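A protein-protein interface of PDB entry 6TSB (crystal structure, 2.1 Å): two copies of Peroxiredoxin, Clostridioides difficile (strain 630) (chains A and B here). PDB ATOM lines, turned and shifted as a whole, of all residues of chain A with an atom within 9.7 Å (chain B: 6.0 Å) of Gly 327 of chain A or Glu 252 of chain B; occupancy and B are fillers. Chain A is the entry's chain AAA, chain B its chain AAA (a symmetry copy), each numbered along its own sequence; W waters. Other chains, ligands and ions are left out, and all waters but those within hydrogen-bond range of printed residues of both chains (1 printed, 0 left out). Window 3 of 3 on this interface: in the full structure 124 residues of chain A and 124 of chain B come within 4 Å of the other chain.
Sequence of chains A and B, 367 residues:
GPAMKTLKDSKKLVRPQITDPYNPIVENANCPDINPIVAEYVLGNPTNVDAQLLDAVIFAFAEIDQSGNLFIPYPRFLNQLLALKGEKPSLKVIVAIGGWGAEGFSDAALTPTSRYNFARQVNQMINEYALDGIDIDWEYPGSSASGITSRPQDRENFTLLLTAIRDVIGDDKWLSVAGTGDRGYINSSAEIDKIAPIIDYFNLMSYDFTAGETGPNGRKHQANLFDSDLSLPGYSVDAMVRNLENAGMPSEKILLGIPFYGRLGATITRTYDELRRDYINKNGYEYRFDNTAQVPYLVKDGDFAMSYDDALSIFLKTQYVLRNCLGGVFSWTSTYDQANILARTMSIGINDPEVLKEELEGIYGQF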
ATOM      1  N   THR A 318       8.996   7.498  17.011  1.00  0.00           N
ATOM      2  CA  THR A 318       9.230   6.046  17.212  1.00  0.00           C
ATOM      3  C   THR A 318      10.012   5.818  18.515  1.00  0.00           C
ATOM      4  O   THR A 318       9.862   4.716  19.128  1.00  0.00           O
ATOM      5  CB  THR A 318       9.947   5.401  16.010  1.00  0.00           C
ATOM      6  OG1 THR A 318      11.104   6.154  15.630  1.00  0.00           O
ATOM      7  CG2 THR A 318       9.030   5.242  14.808  1.00  0.00           C
ATOM      8  N   TYR A 320       9.496   7.739  21.268  1.00  0.00           N
ATOM      9  CA  TYR A 320       8.368   7.920  22.211  1.00  0.00           C
ATOM     10  C   TYR A 320       7.629   6.588  22.342  1.00  0.00           C
ATOM     11  O   TYR A 320       7.252   6.228  23.450  1.00  0.00           O
ATOM     12  CB  TYR A 320       7.492   9.090  21.767  1.00  0.00           C
ATOM     13  CG  TYR A 320       6.418   9.485  22.743  1.00  0.00           C
ATOM     14  CD1 TYR A 320       5.245   8.746  22.883  1.00  0.00           C
ATOM     15  CD2 TYR A 320       6.563  10.629  23.526  1.00  0.00           C
ATOM     16  CE1 TYR A 320       4.255   9.136  23.779  1.00  0.00           C
ATOM     17  CE2 TYR A 320       5.577  11.033  24.419  1.00  0.00           C
ATOM     18  CZ  TYR A 320       4.415  10.290  24.543  1.00  0.00           C
ATOM     19  OH  TYR A 320       3.470  10.714  25.441  1.00  0.00           O
ATOM     20  N   VAL A 321       7.459   5.863  21.239  1.00  0.00           N
ATOM     21  CA  VAL A 321       6.719   4.575  21.230  1.00  0.00           C
ATOM     22  C   VAL A 321       7.482   3.604  22.133  1.00  0.00           C
ATOM     23  O   VAL A 321       6.863   2.832  22.917  1.00  0.00           O
ATOM     24  CB  VAL A 321       6.528   4.039  19.787  1.00  0.00           C
ATOM     25  CG1 VAL A 321       6.261   2.540  19.742  1.00  0.00           C
ATOM     26  CG2 VAL A 321       5.414   4.774  19.057  1.00  0.00           C
ATOM     27  N   LEU A 322       8.791   3.585  21.980  1.00  0.00           N
ATOM     28  CA  LEU A 322       9.642   2.564  22.630  1.00  0.00           C
ATOM     29  C   LEU A 322       9.855   2.966  24.097  1.00  0.00           C
ATOM     30  O   LEU A 322       9.876   2.091  24.936  1.00  0.00           O
ATOM     31  CB  LEU A 322      10.954   2.481  21.848  1.00  0.00           C
ATOM     32  CG  LEU A 322      10.840   1.854  20.455  1.00  0.00           C
ATOM     33  CD1 LEU A 322      11.964   2.358  19.565  1.00  0.00           C
ATOM     34  CD2 LEU A 322      10.853   0.324  20.548  1.00  0.00           C
ATOM     35  N   ARG A 323      10.007   4.251  24.398  1.00  0.00           N
ATOM     36  CA  ARG A 323      10.327   4.654  25.788  1.00  0.00           C
ATOM     37  C   ARG A 323       9.026   4.467  26.579  1.00  0.00           C
ATOM     38  O   ARG A 323       9.122   3.827  27.646  1.00  0.00           O
ATOM     39  CB  ARG A 323      11.083   5.993  25.844  1.00  0.00           C
ATOM     40  CG  ARG A 323      10.325   7.204  26.368  1.00  0.00           C
ATOM     41  CD  ARG A 323      11.253   8.404  26.573  1.00  0.00           C
ATOM     42  NE  ARG A 323      11.892   8.835  25.330  1.00  0.00           N
ATOM     43  CZ  ARG A 323      11.385   9.708  24.452  1.00  0.00           C
ATOM     44  NH1 ARG A 323      12.053   9.988  23.344  1.00  0.00           N
ATOM     45  NH2 ARG A 323      10.233  10.318  24.680  1.00  0.00           N
ATOM     46  N   ASN A 324       7.862   4.773  25.978  1.00  0.00           N
ATOM     47  CA  ASN A 324       6.533   4.796  26.650  1.00  0.00           C
ATOM     48  C   ASN A 324       5.733   3.482  26.545  1.00  0.00           C
ATOM     49  O   ASN A 324       4.534   3.481  26.990  1.00  0.00           O
ATOM     50  CB  ASN A 324       5.745   5.989  26.147  1.00  0.00           C
ATOM     51  CG  ASN A 324       6.351   7.274  26.650  1.00  0.00           C
ATOM     52  OD1 ASN A 324       6.957   8.013  25.883  1.00  0.00           O
ATOM     53  ND2 ASN A 324       6.173   7.551  27.937  1.00  0.00           N
ATOM     54  N   CYS A 325       6.351   2.380  26.101  1.00  0.00           N
ATOM     55  CA  CYS A 325       5.739   1.022  26.021  1.00  0.00           C
ATOM     56  C   CYS A 325       4.398   1.049  25.261  1.00  0.00           C
ATOM     57  O   CYS A 325       3.449   0.355  25.690  1.00  0.00           O
ATOM     58  CB  CYS A 325       5.627   0.456  27.431  1.00  0.00           C
ATOM     59  SG  CYS A 325       7.270   0.260  28.192  1.00  0.00           S
ATOM     60  N   LEU A 326       4.321   1.781  24.137  1.00  0.00           N
ATOM     61  CA  LEU A 326       3.130   1.755  23.239  1.00  0.00           C
ATOM     62  C   LEU A 326       3.140   0.490  22.362  1.00  0.00           C
ATOM     63  O   LEU A 326       4.131  -0.262  22.340  1.00  0.00           O
ATOM     64  CB  LEU A 326       3.067   3.012  22.363  1.00  0.00           C
ATOM     65  CG  LEU A 326       3.091   4.380  23.056  1.00  0.00           C
ATOM     66  CD1 LEU A 326       2.519   5.446  22.124  1.00  0.00           C
ATOM     67  CD2 LEU A 326       2.334   4.401  24.374  1.00  0.00           C
ATOM     68  N   GLY A 327       2.036   0.241  21.659  1.00  0.00           N
ATOM     69  CA  GLY A 327       1.843  -0.998  20.877  1.00  0.00           C
ATOM     70  C   GLY A 327       2.546  -0.966  19.519  1.00  0.00           C
ATOM     71  O   GLY A 327       2.850  -2.014  18.987  1.00  0.00           O
ATOM     72  N   GLY A 328       2.851   0.207  18.993  1.00  0.00           N
ATOM     73  CA  GLY A 328       3.539   0.304  17.705  1.00  0.00           C
ATOM     74  C   GLY A 328       3.174   1.609  17.092  1.00  0.00           C
ATOM     75  O   GLY A 328       2.676   2.502  17.819  1.00  0.00           O
ATOM     76  N   VAL A 329       3.348   1.704  15.787  1.00  0.00           N
ATOM     77  CA  VAL A 329       3.150   2.954  15.022  1.00  0.00           C
ATOM     78  C   VAL A 329       2.448   2.570  13.715  1.00  0.00           C
ATOM     79  O   VAL A 329       2.449   1.387  13.352  1.00  0.00           O
ATOM     80  CB  VAL A 329       4.533   3.593  14.807  1.00  0.00           C
ATOM     81  CG1 VAL A 329       5.410   2.747  13.909  1.00  0.00           C
ATOM     82  CG2 VAL A 329       4.449   5.007  14.273  1.00  0.00           C
ATOM     83  N   PHE A 330       1.864   3.545  13.045  1.00  0.00           N
ATOM     84  CA  PHE A 330       1.108   3.380  11.792  1.00  0.00           C
ATOM     85  C   PHE A 330       1.187   4.717  11.087  1.00  0.00           C
ATOM     86  O   PHE A 330       1.372   5.718  11.781  1.00  0.00           O
ATOM     87  CB  PHE A 330      -0.349   2.950  12.042  1.00  0.00           C
ATOM     88  CG  PHE A 330      -1.342   4.016  12.467  1.00  0.00           C
ATOM     89  CD1 PHE A 330      -1.912   4.875  11.539  1.00  0.00           C
ATOM     90  CD2 PHE A 330      -1.728   4.152  13.807  1.00  0.00           C
ATOM     91  CE1 PHE A 330      -2.855   5.822  11.911  1.00  0.00           C
ATOM     92  CE2 PHE A 330      -2.660   5.106  14.192  1.00  0.00           C
ATOM     93  CZ  PHE A 330      -3.220   5.948  13.245  1.00  0.00           C
ATOM     94  N   ILE A 350      11.344   1.803  14.753  1.00  0.00           N
ATOM     95  CA  ILE A 350      10.850   0.718  15.649  1.00  0.00           C
ATOM     96  C   ILE A 350      11.806  -0.476  15.659  1.00  0.00           C
ATOM     97  O   ILE A 350      11.986  -1.037  16.747  1.00  0.00           O
ATOM     98  CB  ILE A 350       9.434   0.245  15.224  1.00  0.00           C
ATOM     99  CG1 ILE A 350       8.397   1.364  15.342  1.00  0.00           C
ATOM    100  CG2 ILE A 350       9.014  -0.993  16.000  1.00  0.00           C
ATOM    101  CD1 ILE A 350       8.305   1.986  16.714  1.00  0.00           C
ATOM    102  N   ILE B  34       5.908  -7.274  24.884  1.00  0.00           N
ATOM    103  CA  ILE B  34       5.500  -6.102  24.037  1.00  0.00           C
ATOM    104  C   ILE B  34       6.464  -6.090  22.854  1.00  0.00           C
ATOM    105  O   ILE B  34       7.629  -5.712  23.045  1.00  0.00           O
ATOM    106  CB  ILE B  34       5.448  -4.720  24.744  1.00  0.00           C
ATOM    107  CG1 ILE B  34       4.352  -4.651  25.816  1.00  0.00           C
ATOM    108  CG2 ILE B  34       5.272  -3.590  23.725  1.00  0.00           C
ATOM    109  CD1 ILE B  34       4.540  -3.546  26.847  1.00  0.00           C
ATOM    110  N   ASN B  35       5.969  -6.510  21.691  1.00  0.00           N
ATOM    111  CA  ASN B  35       6.730  -6.646  20.422  1.00  0.00           C
ATOM    112  C   ASN B  35       6.186  -5.634  19.413  1.00  0.00           C
ATOM    113  O   ASN B  35       5.454  -6.012  18.510  1.00  0.00           O
ATOM    114  CB  ASN B  35       6.629  -8.093  19.926  1.00  0.00           C
ATOM    115  CG  ASN B  35       7.984  -8.732  19.712  1.00  0.00           C
ATOM    116  OD1 ASN B  35       8.284  -9.777  20.297  1.00  0.00           O
ATOM    117  ND2 ASN B  35       8.805  -8.097  18.891  1.00  0.00           N
ATOM    118  N   PRO B  36       6.563  -4.335  19.484  1.00  0.00           N
ATOM    119  CA  PRO B  36       5.778  -3.259  18.878  1.00  0.00           C
ATOM    120  C   PRO B  36       5.799  -3.320  17.345  1.00  0.00           C
ATOM    121  O   PRO B  36       6.818  -3.663  16.793  1.00  0.00           O
ATOM    122  CB  PRO B  36       6.439  -1.968  19.372  1.00  0.00           C
ATOM    123  CG  PRO B  36       7.874  -2.369  19.609  1.00  0.00           C
ATOM    124  CD  PRO B  36       7.832  -3.828  20.027  1.00  0.00           C
ATOM    125  N   ILE B  37       4.657  -3.013  16.729  1.00  0.00           N
ATOM    126  CA  ILE B  37       4.339  -3.387  15.328  1.00  0.00           C
ATOM    127  C   ILE B  37       4.359  -2.122  14.493  1.00  0.00           C
ATOM    128  O   ILE B  37       4.241  -1.002  15.060  1.00  0.00           O
ATOM    129  CB  ILE B  37       2.995  -4.128  15.186  1.00  0.00           C
ATOM    130  CG1 ILE B  37       1.786  -3.260  15.533  1.00  0.00           C
ATOM    131  CG2 ILE B  37       2.981  -5.438  15.955  1.00  0.00           C
ATOM    132  CD1 ILE B  37       0.465  -3.922  15.163  1.00  0.00           C
ATOM    133  N   ASP B 200      -8.085  -4.967  20.178  1.00  0.00           N
ATOM    134  CA  ASP B 200      -6.654  -5.358  20.174  1.00  0.00           C
ATOM    135  C   ASP B 200      -5.807  -4.088  20.155  1.00  0.00           C
ATOM    136  O   ASP B 200      -4.766  -4.060  20.816  1.00  0.00           O
ATOM    137  CB  ASP B 200      -6.331  -6.244  18.979  1.00  0.00           C
ATOM    138  CG  ASP B 200      -7.016  -7.590  19.063  1.00  0.00           C
ATOM    139  OD1 ASP B 200      -6.572  -8.395  19.851  1.00  0.00           O
ATOM    140  OD2 ASP B 200      -8.006  -7.800  18.365  1.00  0.00           O
ATOM    141  N   TYR B 201      -6.258  -3.053  19.465  1.00  0.00           N
ATOM    142  CA  TYR B 201      -5.496  -1.798  19.323  1.00  0.00           C
ATOM    143  C   TYR B 201      -6.454  -0.619  19.249  1.00  0.00           C
ATOM    144  O   TYR B 201      -7.557  -0.769  18.721  1.00  0.00           O
ATOM    145  CB  TYR B 201      -4.622  -1.837  18.066  1.00  0.00           C
ATOM    146  CG  TYR B 201      -3.515  -2.858  18.112  1.00  0.00           C
ATOM    147  CD1 TYR B 201      -2.391  -2.648  18.895  1.00  0.00           C
ATOM    148  CD2 TYR B 201      -3.562  -4.017  17.359  1.00  0.00           C
ATOM    149  CE1 TYR B 201      -1.373  -3.591  18.972  1.00  0.00           C
ATOM    150  CE2 TYR B 201      -2.534  -4.950  17.384  1.00  0.00           C
ATOM    151  CZ  TYR B 201      -1.442  -4.736  18.204  1.00  0.00           C
ATOM    152  OH  TYR B 201      -0.412  -5.616  18.239  1.00  0.00           O
ATOM    153  N   PRO B 250      -4.651   0.548  28.029  1.00  0.00           N
ATOM    154  CA  PRO B 250      -3.291   0.058  28.243  1.00  0.00           C
ATOM    155  C   PRO B 250      -2.345   0.659  27.193  1.00  0.00           C
ATOM    156  O   PRO B 250      -2.765   0.918  26.042  1.00  0.00           O
ATOM    157  CB  PRO B 250      -3.372  -1.461  28.036  1.00  0.00           C
ATOM    158  CG  PRO B 250      -4.828  -1.806  28.196  1.00  0.00           C
ATOM    159  CD  PRO B 250      -5.615  -0.545  27.884  1.00  0.00           C
ATOM    160  N   SER B 251      -1.090   0.885  27.570  1.00  0.00           N
ATOM    161  CA  SER B 251      -0.138   1.589  26.690  1.00  0.00           C
ATOM    162  C   SER B 251       0.109   0.726  25.428  1.00  0.00           C
ATOM    163  O   SER B 251       0.092   1.308  24.343  1.00  0.00           O
ATOM    164  CB  SER B 251       1.115   1.970  27.451  1.00  0.00           C
ATOM    165  OG  SER B 251       1.819   0.803  27.884  1.00  0.00           O
ATOM    166  N   GLU B 252       0.294  -0.589  25.605  1.00  0.00           N
ATOM    167  CA  GLU B 252       0.639  -1.648  24.617  1.00  0.00           C
ATOM    168  C   GLU B 252      -0.405  -1.780  23.499  1.00  0.00           C
ATOM    169  O   GLU B 252      -0.159  -2.609  22.607  1.00  0.00           O
ATOM    170  CB  GLU B 252       0.578  -3.076  25.187  1.00  0.00           C
ATOM    171  CG  GLU B 252       1.075  -3.274  26.592  1.00  0.00           C
ATOM    172  CD  GLU B 252       0.062  -3.026  27.704  1.00  0.00           C
ATOM    173  OE1 GLU B 252      -0.690  -3.977  28.055  1.00  0.00           O
ATOM    174  OE2 GLU B 252       0.047  -1.877  28.233  1.00  0.00           O
ATOM    175  N   LYS B 253      -1.597  -1.202  23.674  1.00  0.00           N
ATOM    176  CA  LYS B 253      -2.727  -1.320  22.718  1.00  0.00           C
ATOM    177  C   LYS B 253      -2.815  -0.007  21.944  1.00  0.00           C
ATOM    178  O   LYS B 253      -3.560   0.030  20.968  1.00  0.00           O
ATOM    179  CB  LYS B 253      -4.046  -1.668  23.434  1.00  0.00           C
ATOM    180  CG  LYS B 253      -4.159  -3.108  23.962  1.00  0.00           C
ATOM    181  CD  LYS B 253      -5.576  -3.516  24.380  1.00  0.00           C
ATOM    182  CE  LYS B 253      -5.704  -4.973  24.777  1.00  0.00           C
ATOM    183  NZ  LYS B 253      -7.089  -5.317  25.200  1.00  0.00           N
ATOM    184  N   ILE B 254      -2.046   1.018  22.335  1.00  0.00           N
ATOM    185  CA  ILE B 254      -2.031   2.294  21.583  1.00  0.00           C
ATOM    186  C   ILE B 254      -1.059   2.209  20.405  1.00  0.00           C
ATOM    187  O   ILE B 254       0.131   1.947  20.654  1.00  0.00           O
ATOM    188  CB  ILE B 254      -1.672   3.478  22.463  1.00  0.00           C
ATOM    189  CG1 ILE B 254      -2.592   3.517  23.686  1.00  0.00           C
ATOM    190  CG2 ILE B 254      -1.713   4.738  21.590  1.00  0.00           C
ATOM    191  CD1 ILE B 254      -2.648   4.854  24.377  1.00  0.00           C
ATOM    192  N   LEU B 255      -1.548   2.503  19.194  1.00  0.00           N
ATOM    193  CA  LEU B 255      -0.700   2.637  17.980  1.00  0.00           C
ATOM    194  C   LEU B 255      -0.601   4.103  17.650  1.00  0.00           C
ATOM    195  O   LEU B 255      -1.677   4.734  17.500  1.00  0.00           O
ATOM    196  CB  LEU B 255      -1.333   1.903  16.806  1.00  0.00           C
ATOM    197  CG  LEU B 255      -1.386   0.389  16.933  1.00  0.00           C
ATOM    198  CD1 LEU B 255      -1.668  -0.234  15.571  1.00  0.00           C
ATOM    199  CD2 LEU B 255      -0.102  -0.150  17.538  1.00  0.00           C
HETATM  200  O   HOH W   1       1.987  -4.221  19.421  1.00  0.00           O
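Printed residues of chain A that touch a printed residue of chain B: Asn 324, Cys 325, Leu 326, Gly 327, Gly 328, Val 329, Phe 330 and Ile 350. Hydrophobic or aromatic side chains of chain A within 4 Å of the printed part of chain B: Leu 326, Phe 330 and Ile 350. Among the printed residues, 19 pairs touch across the chains.
Gly 327 of chain A touches just these residues of chain B: Pro 36 (3.2 Å), Ile 37 (3.1 Å), Ser 251 (3.5 Å), Glu 252 (3.1 Å), Ile 254 (2.7 Å) and Leu 255 (3.4 Å). Of the printed residues of chain B, Gly 328 of chain A touches Ile 37 (3.0 Å), Ile 254 (3.6 Å) and Leu 255 (3.3 Å). Printed residues of chain B within 4 Å of Val 329 of chain A: Ile 37. Of the printed residues of chain B, Phe 330 of chain A touches Leu 255 (3.5 Å). Of the printed residues of chain B, Ile 350 of chain A touches Pro 36. Printed residues of chain A within 4 Å of Ile 34 of chain B: Leu 326. Pro 36 of chain B touches just these residues of chain A: Gly 327 and Ile 350. Ile 37 of chain B touches just these residues of chain A: Gly 327, Gly 328 and Val 329. Printed residues of chain A within 4 Å of Glu 252 of chain B: Cys 325 (3.3 Å), Leu 326 (3.99 Å) and Gly 327 (3.1 Å). The nearest residue of chain B that does not touch Gly 327 of chain A is Lys 253 of chain B (4.4 Å). The nearest printed residue of chain A that does not touch Ile 254 of chain B is Val 329 of chain A (5.8 Å).
The backbone carbonyl oxygen (O) of Val 321 of chain A sits at hydrogen-bond distance from the backbone NH (N) of Leu 326 of chain A (3.0 Å). The backbone carbonyl oxygen of Tyr 320 of chain A lies close to the side-chain amide oxygen of Asn 324 of chain A (3.0 Å). The side-chain carboxylate (OE2) of Glu 252 of chain B sits at hydrogen-bond distance from the side-chain hydroxyl (OG) of Ser 251 of chain B.
Water W1 lies within hydrogen-bond range of the backbone carbonyl oxygen (O) of Gly 327 of chain A (2.4 Å) and the side-chain hydroxyl (OH) of Tyr 201 of chain B (3.0 Å).
Among the printed residues, merely in contact across the chains: Gly 328 of chain A with Ile 37 of chain B, Gly 327 of chain A with Glu 252 of chain B, Gly 327 of chain A with Pro 36 of chain B, Leu 326 of chain A with Ser 251 of chain B, Gly 328 of chain A with Leu 255 of chain B, Gly 327 of chain A with Leu 255 of chain B, Phe 330 of chain A with Leu 255 of chain B, Ile 350 of chain A with Pro 36 of chain B, Leu 326 of chain A with Ile 254 of chain B, Gly 328 of chain A with Ile 254 of chain B, Asn 324 of chain A with Ser 251 of chain B, Leu 326 of chain A with Ile 34 of chain B and Leu 326 of chain A with Glu 252 of chain B.
N of Gly 327 of chain A sits at hydrogen-bond distance from O of Ile 254 of chain B. The backbone carbonyl oxygen (O) of Cys 325 of chain A sits at hydrogen-bond distance from the side-chain hydroxyl (OG) of Ser 251 of chain B, 2.8 Å away. The backbone carbonyl oxygen (O) of Gly 327 of chain A sits at hydrogen-bond distance from the backbone NH (N) of Ile 37 of chain B, at 3.1 Å. The backbone NH (N) of Val 329 of chain A sits at hydrogen-bond distance from the backbone carbonyl oxygen (O) of Ile 37 of chain B. N of Glu 252 of chain B sits at hydrogen-bond distance from O of Cys 325 of chain A (3.3 Å). N of Gly 327 of chain A is in hydrogen-bond range of O of Ser 251 of chain B (3.5 Å).
No position is printed for both chains.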
